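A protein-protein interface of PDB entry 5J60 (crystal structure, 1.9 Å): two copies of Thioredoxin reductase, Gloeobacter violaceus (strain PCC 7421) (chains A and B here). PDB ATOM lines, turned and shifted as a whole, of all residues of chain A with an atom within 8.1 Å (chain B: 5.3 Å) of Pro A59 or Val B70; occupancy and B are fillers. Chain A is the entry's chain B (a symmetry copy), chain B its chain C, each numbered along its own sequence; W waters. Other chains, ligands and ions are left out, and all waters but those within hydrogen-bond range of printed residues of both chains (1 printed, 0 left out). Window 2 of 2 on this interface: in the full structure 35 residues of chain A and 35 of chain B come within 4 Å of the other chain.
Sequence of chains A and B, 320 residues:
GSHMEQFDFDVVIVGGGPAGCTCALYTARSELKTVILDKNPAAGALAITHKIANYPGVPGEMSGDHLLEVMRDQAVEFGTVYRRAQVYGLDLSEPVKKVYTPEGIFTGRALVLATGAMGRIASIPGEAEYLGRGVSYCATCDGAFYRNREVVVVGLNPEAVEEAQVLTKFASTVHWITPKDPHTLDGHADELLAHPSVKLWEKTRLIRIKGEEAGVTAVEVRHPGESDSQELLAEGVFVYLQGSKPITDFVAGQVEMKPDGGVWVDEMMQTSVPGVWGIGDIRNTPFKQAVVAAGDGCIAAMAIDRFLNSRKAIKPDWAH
The side-chain amide nitrogen of Gln B74 lies within hydrogen-bond range of the backbone carbonyl oxygen of Tyr A55 (3.1 Å). The side-chain amide nitrogen of Gln B74 is in hydrogen-bond range of the backbone carbonyl oxygen of Val A58 (3.3 Å). The side-chain amide oxygen (OE1) of Gln B74 lies within hydrogen-bond range of the backbone NH (N) of Gly A57 (2.7 Å).
Among the printed residues, merely in contact across the chains: Pro A56 with Gln B74 (3.4 Å), Gly A57 with Val B70 (3.5 Å), Gly A57 with Met B71 (3.6 Å), Pro A59 with Val B70 (3.7 Å) and Gly A57 with Leu B67 (3.8 Å).
Of the printed residues of chain B, Pro A59 touches Val B70 (3.7 Å). Val B70 touches just these residues of chain A: Gly A57 and Pro A59. Of the printed residues of chain A, Leu B67 touches Gly A57 (3.8 Å). Of the printed residues of chain B, Gly A57 touches Leu B67 (3.8 Å), Val B70 (3.5 Å), Met B71 (3.6 Å) and Gln B74 (2.7 Å). Gly A60 touches none of the printed residues of chain B. The nearest residue of chain A that does not touch Val B70 is Val A58 (4.2 Å).
Of the 11 printed residues of chain A, 5 touch a printed residue of chain B. Of the 11 printed residues of chain B, 4 touch a printed residue of chain A. Hydrophobic or aromatic side chains of chain B within 4 Å of the printed part of chain A: Leu B67, Val B70 and Met B71. Along chain B the printed residues that touch a printed residue of chain A span positions 67 to 74. Among the printed residues, no Asp or Glu carboxylate lies within 4 Å of a Lys or Arg side-chain nitrogen of the other chain.
No position is printed for both chains.
Water W1 bridges the backbone carbonyl oxygen of Ala A53 and the side-chain amide nitrogen of Gln B74.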
ATOM      1  N   ILE A  52     -36.363  -3.011   1.443  1.00  0.00           N
ATOM      2  CA  ILE A  52     -35.902  -2.018   0.480  1.00  0.00           C
ATOM      3  C   ILE A  52     -35.770  -2.682  -0.881  1.00  0.00           C
ATOM      4  O   ILE A  52     -35.091  -3.710  -1.023  1.00  0.00           O
ATOM      5  CB  ILE A  52     -34.588  -1.359   0.933  1.00  0.00           C
ATOM      6  CG1 ILE A  52     -34.138  -0.295  -0.086  1.00  0.00           C
ATOM      7  CG2 ILE A  52     -33.468  -2.377   1.137  1.00  0.00           C
ATOM      8  CD1 ILE A  52     -33.020   0.647   0.476  1.00  0.00           C
ATOM      9  N   ALA A  53     -36.431  -2.092  -1.882  1.00  0.00           N
ATOM     10  CA  ALA A  53     -36.480  -2.637  -3.233  1.00  0.00           C
ATOM     11  C   ALA A  53     -35.955  -1.668  -4.283  1.00  0.00           C
ATOM     12  O   ALA A  53     -36.032  -1.968  -5.474  1.00  0.00           O
ATOM     13  CB  ALA A  53     -37.921  -3.045  -3.580  1.00  0.00           C
ATOM     14  N   ASN A  54     -35.417  -0.520  -3.882  1.00  0.00           N
ATOM     15  CA  ASN A  54     -34.947   0.456  -4.860  1.00  0.00           C
ATOM     16  C   ASN A  54     -33.505   0.843  -4.601  1.00  0.00           C
ATOM     17  O   ASN A  54     -33.069   1.931  -4.978  1.00  0.00           O
ATOM     18  CB  ASN A  54     -35.837   1.697  -4.868  1.00  0.00           C
ATOM     19  CG  ASN A  54     -35.986   2.310  -3.505  1.00  0.00           C
ATOM     20  OD1 ASN A  54     -35.272   1.958  -2.567  1.00  0.00           O
ATOM     21  ND2 ASN A  54     -36.904   3.259  -3.391  1.00  0.00           N
ATOM     22  N   TYR A  55     -32.737  -0.044  -3.974  1.00  0.00           N
ATOM     23  CA  TYR A  55     -31.305   0.175  -3.879  1.00  0.00           C
ATOM     24  C   TYR A  55     -30.665  -0.450  -5.103  1.00  0.00           C
ATOM     25  O   TYR A  55     -30.687  -1.693  -5.243  1.00  0.00           O
ATOM     26  CB  TYR A  55     -30.723  -0.419  -2.614  1.00  0.00           C
ATOM     27  CG  TYR A  55     -29.286   0.010  -2.432  1.00  0.00           C
ATOM     28  CD1 TYR A  55     -28.982   1.233  -1.889  1.00  0.00           C
ATOM     29  CD2 TYR A  55     -28.235  -0.803  -2.840  1.00  0.00           C
ATOM     30  CE1 TYR A  55     -27.679   1.641  -1.740  1.00  0.00           C
ATOM     31  CE2 TYR A  55     -26.925  -0.404  -2.683  1.00  0.00           C
ATOM     32  CZ  TYR A  55     -26.659   0.820  -2.143  1.00  0.00           C
ATOM     33  OH  TYR A  55     -25.366   1.242  -1.970  1.00  0.00           O
ATOM     34  N   PRO A  56     -30.094   0.337  -6.002  1.00  0.00           N
ATOM     35  CA  PRO A  56     -29.617  -0.232  -7.262  1.00  0.00           C
ATOM     36  C   PRO A  56     -28.467  -1.201  -7.033  1.00  0.00           C
ATOM     37  O   PRO A  56     -27.517  -0.907  -6.302  1.00  0.00           O
ATOM     38  CB  PRO A  56     -29.185   1.007  -8.065  1.00  0.00           C
ATOM     39  CG  PRO A  56     -29.037   2.050  -7.146  1.00  0.00           C
ATOM     40  CD  PRO A  56     -29.916   1.797  -5.958  1.00  0.00           C
ATOM     41  N   GLY A  57     -28.561  -2.355  -7.674  1.00  0.00           N
ATOM     42  CA  GLY A  57     -27.556  -3.386  -7.555  1.00  0.00           C
ATOM     43  C   GLY A  57     -27.855  -4.457  -6.529  1.00  0.00           C
ATOM     44  O   GLY A  57     -27.141  -5.466  -6.500  1.00  0.00           O
ATOM     45  N   VAL A  58     -28.902  -4.286  -5.726  1.00  0.00           N
ATOM     46  CA  VAL A  58     -29.301  -5.249  -4.699  1.00  0.00           C
ATOM     47  C   VAL A  58     -30.709  -5.712  -5.040  1.00  0.00           C
ATOM     48  O   VAL A  58     -31.683  -5.040  -4.676  1.00  0.00           O
ATOM     49  CB  VAL A  58     -29.231  -4.632  -3.290  1.00  0.00           C
ATOM     50  CG1 VAL A  58     -29.764  -5.604  -2.246  1.00  0.00           C
ATOM     51  CG2 VAL A  58     -27.797  -4.254  -2.946  1.00  0.00           C
ATOM     52  N   PRO A  59     -30.866  -6.826  -5.756  1.00  0.00           N
ATOM     53  CA  PRO A  59     -32.188  -7.230  -6.231  1.00  0.00           C
ATOM     54  C   PRO A  59     -32.953  -8.025  -5.183  1.00  0.00           C
ATOM     55  O   PRO A  59     -32.428  -8.409  -4.140  1.00  0.00           O
ATOM     56  CB  PRO A  59     -31.862  -8.105  -7.436  1.00  0.00           C
ATOM     57  CG  PRO A  59     -30.604  -8.788  -7.045  1.00  0.00           C
ATOM     58  CD  PRO A  59     -29.830  -7.790  -6.177  1.00  0.00           C
ATOM     59  N   GLY A  60     -34.212  -8.294  -5.501  1.00  0.00           N
ATOM     60  CA  GLY A  60     -34.998  -9.195  -4.688  1.00  0.00           C
ATOM     61  C   GLY A  60     -35.481  -8.584  -3.382  1.00  0.00           C
ATOM     62  O   GLY A  60     -35.648  -7.369  -3.234  1.00  0.00           O
ATOM     63  N   GLU A  61     -35.728  -9.464  -2.417  1.00  0.00           N
ATOM     64  CA  GLU A  61     -36.222  -9.030  -1.121  1.00  0.00           C
ATOM     65  C   GLU A  61     -35.026  -8.843  -0.202  1.00  0.00           C
ATOM     66  O   GLU A  61     -34.219  -9.766  -0.033  1.00  0.00           O
ATOM     67  CB  GLU A  61     -37.200 -10.055  -0.544  1.00  0.00           C
ATOM     68  N   MET A  62     -34.890  -7.643   0.364  1.00  0.00           N
ATOM     69  CA  MET A  62     -33.864  -7.436   1.374  1.00  0.00           C
ATOM     70  C   MET A  62     -34.367  -6.466   2.428  1.00  0.00           C
ATOM     71  O   MET A  62     -34.947  -5.430   2.113  1.00  0.00           O
ATOM     72  CB  MET A  62     -32.557  -6.919   0.771  1.00  0.00           C
ATOM     73  CG  MET A  62     -31.454  -6.861   1.821  1.00  0.00           C
ATOM     74  SD  MET A  62     -29.768  -6.793   1.228  1.00  0.00           S
ATOM     75  CE  MET A  62     -29.651  -8.267   0.190  1.00  0.00           C
ATOM     76  N   ASP B  65     -19.823  -5.682 -15.287  1.00  0.00           N
ATOM     77  CA  ASP B  65     -20.992  -5.874 -16.135  1.00  0.00           C
ATOM     78  C   ASP B  65     -22.057  -6.721 -15.459  1.00  0.00           C
ATOM     79  O   ASP B  65     -23.222  -6.646 -15.859  1.00  0.00           O
ATOM     80  CB  ASP B  65     -20.635  -6.435 -17.520  1.00  0.00           C
ATOM     81  CG  ASP B  65     -19.942  -7.770 -17.489  1.00  0.00           C
ATOM     82  OD1 ASP B  65     -19.822  -8.387 -16.416  1.00  0.00           O
ATOM     83  OD2 ASP B  65     -19.527  -8.210 -18.586  1.00  0.00           O
ATOM     84  N   HIS B  66     -21.702  -7.501 -14.434  1.00  0.00           N
ATOM     85  CA  HIS B  66     -22.733  -8.200 -13.669  1.00  0.00           C
ATOM     86  C   HIS B  66     -23.477  -7.243 -12.752  1.00  0.00           C
ATOM     87  O   HIS B  66     -24.703  -7.317 -12.634  1.00  0.00           O
ATOM     88  CB  HIS B  66     -22.135  -9.347 -12.861  1.00  0.00           C
ATOM     89  CG  HIS B  66     -23.161 -10.121 -12.094  1.00  0.00           C
ATOM     90  ND1 HIS B  66     -23.272 -10.066 -10.721  1.00  0.00           N
ATOM     91  CD2 HIS B  66     -24.169 -10.916 -12.517  1.00  0.00           C
ATOM     92  CE1 HIS B  66     -24.274 -10.834 -10.329  1.00  0.00           C
ATOM     93  NE2 HIS B  66     -24.837 -11.360 -11.400  1.00  0.00           N
ATOM     94  N   LEU B  67     -22.760  -6.333 -12.093  1.00  0.00           N
ATOM     95  CA  LEU B  67     -23.444  -5.316 -11.295  1.00  0.00           C
ATOM     96  C   LEU B  67     -24.391  -4.494 -12.169  1.00  0.00           C
ATOM     97  O   LEU B  67     -25.559  -4.264 -11.815  1.00  0.00           O
ATOM     98  CB  LEU B  67     -22.415  -4.409 -10.608  1.00  0.00           C
ATOM     99  CG  LEU B  67     -23.004  -3.240  -9.808  1.00  0.00           C
ATOM    100  CD1 LEU B  67     -23.942  -3.757  -8.714  1.00  0.00           C
ATOM    101  CD2 LEU B  67     -21.880  -2.416  -9.220  1.00  0.00           C
ATOM    102  N   LEU B  68     -23.914  -4.067 -13.343  1.00  0.00           N
ATOM    103  CA  LEU B  68     -24.770  -3.292 -14.226  1.00  0.00           C
ATOM    104  C   LEU B  68     -25.981  -4.103 -14.664  1.00  0.00           C
ATOM    105  O   LEU B  68     -27.087  -3.568 -14.796  1.00  0.00           O
ATOM    106  CB  LEU B  68     -23.977  -2.815 -15.437  1.00  0.00           C
ATOM    107  CG  LEU B  68     -24.733  -1.891 -16.397  1.00  0.00           C
ATOM    108  CD1 LEU B  68     -25.196  -0.633 -15.701  1.00  0.00           C
ATOM    109  CD2 LEU B  68     -23.870  -1.532 -17.579  1.00  0.00           C
ATOM    110  N   GLU B  69     -25.784  -5.394 -14.914  1.00  0.00           N
ATOM    111  CA  GLU B  69     -26.888  -6.250 -15.340  1.00  0.00           C
ATOM    112  C   GLU B  69     -27.998  -6.286 -14.297  1.00  0.00           C
ATOM    113  O   GLU B  69     -29.189  -6.271 -14.641  1.00  0.00           O
ATOM    114  CB  GLU B  69     -26.349  -7.666 -15.597  1.00  0.00           C
ATOM    115  CG  GLU B  69     -27.374  -8.707 -15.937  1.00  0.00           C
ATOM    116  CD  GLU B  69     -26.767 -10.120 -16.117  1.00  0.00           C
ATOM    117  OE1 GLU B  69     -25.701 -10.427 -15.526  1.00  0.00           O
ATOM    118  OE2 GLU B  69     -27.395 -10.942 -16.812  1.00  0.00           O
ATOM    119  N   VAL B  70     -27.624  -6.355 -13.017  1.00  0.00           N
ATOM    120  CA  VAL B  70     -28.601  -6.328 -11.933  1.00  0.00           C
ATOM    121  C   VAL B  70     -29.380  -5.015 -11.947  1.00  0.00           C
ATOM    122  O   VAL B  70     -30.608  -5.006 -11.843  1.00  0.00           O
ATOM    123  CB  VAL B  70     -27.900  -6.548 -10.584  1.00  0.00           C
ATOM    124  CG1 VAL B  70     -28.853  -6.274  -9.453  1.00  0.00           C
ATOM    125  CG2 VAL B  70     -27.370  -7.985 -10.504  1.00  0.00           C
ATOM    126  N   MET B  71     -28.675  -3.887 -12.091  1.00  0.00           N
ATOM    127  CA  MET B  71     -29.333  -2.582 -12.134  1.00  0.00           C
ATOM    128  C   MET B  71     -30.268  -2.483 -13.332  1.00  0.00           C
ATOM    129  O   MET B  71     -31.422  -2.044 -13.209  1.00  0.00           O
ATOM    130  CB  MET B  71     -28.275  -1.477 -12.189  1.00  0.00           C
ATOM    131  CG  MET B  71     -27.371  -1.439 -10.990  1.00  0.00           C
ATOM    132  SD  MET B  71     -26.155  -0.122 -11.246  1.00  0.00           S
ATOM    133  CE  MET B  71     -25.280  -0.116  -9.677  1.00  0.00           C
ATOM    134  N   ARG B  72     -29.791  -2.902 -14.504  1.00  0.00           N
ATOM    135  CA  ARG B  72     -30.637  -2.880 -15.684  1.00  0.00           C
ATOM    136  C   ARG B  72     -31.867  -3.741 -15.473  1.00  0.00           C
ATOM    137  O   ARG B  72     -32.980  -3.343 -15.838  1.00  0.00           O
ATOM    138  CB  ARG B  72     -29.856  -3.357 -16.913  1.00  0.00           C
ATOM    139  CG  ARG B  72     -30.579  -3.135 -18.245  1.00  0.00           C
ATOM    140  CD  ARG B  72     -29.856  -3.808 -19.409  1.00  0.00           C
ATOM    141  NE  ARG B  72     -28.469  -3.354 -19.484  1.00  0.00           N
ATOM    142  CZ  ARG B  72     -27.399  -4.091 -19.193  1.00  0.00           C
ATOM    143  NH1 ARG B  72     -27.514  -5.370 -18.823  1.00  0.00           N
ATOM    144  NH2 ARG B  72     -26.196  -3.539 -19.282  1.00  0.00           N
ATOM    145  N   ASP B  73     -31.682  -4.931 -14.898  1.00  0.00           N
ATOM    146  CA  ASP B  73     -32.808  -5.820 -14.640  1.00  0.00           C
ATOM    147  C   ASP B  73     -33.792  -5.198 -13.654  1.00  0.00           C
ATOM    148  O   ASP B  73     -35.006  -5.347 -13.814  1.00  0.00           O
ATOM    149  CB  ASP B  73     -32.318  -7.179 -14.108  1.00  0.00           C
ATOM    150  CG  ASP B  73     -31.651  -8.041 -15.191  1.00  0.00           C
ATOM    151  OD1 ASP B  73     -31.679  -7.642 -16.381  1.00  0.00           O
ATOM    152  OD2 ASP B  73     -31.109  -9.129 -14.843  1.00  0.00           O
ATOM    153  N   GLN B  74     -33.294  -4.481 -12.637  1.00  0.00           N
ATOM    154  CA  GLN B  74     -34.196  -3.818 -11.696  1.00  0.00           C
ATOM    155  C   GLN B  74     -35.057  -2.778 -12.394  1.00  0.00           C
ATOM    156  O   GLN B  74     -36.278  -2.724 -12.198  1.00  0.00           O
ATOM    157  CB  GLN B  74     -33.402  -3.149 -10.577  1.00  0.00           C
ATOM    158  CG  GLN B  74     -32.901  -4.099  -9.540  1.00  0.00           C
ATOM    159  CD  GLN B  74     -31.980  -3.384  -8.588  1.00  0.00           C
ATOM    160  OE1 GLN B  74     -30.906  -2.911  -8.982  1.00  0.00           O
ATOM    161  NE2 GLN B  74     -32.404  -3.259  -7.344  1.00  0.00           N
ATOM    162  N   ALA B  75     -34.430  -1.939 -13.210  1.00  0.00           N
ATOM    163  CA  ALA B  75     -35.171  -0.894 -13.912  1.00  0.00           C
ATOM    164  C   ALA B  75     -36.267  -1.491 -14.782  1.00  0.00           C
ATOM    165  O   ALA B  75     -37.406  -1.009 -14.775  1.00  0.00           O
ATOM    166  CB  ALA B  75     -34.213  -0.054 -14.753  1.00  0.00           C
HETATM  167  O   HOH W   1     -35.073  -4.304  -6.451  1.00  0.00           O
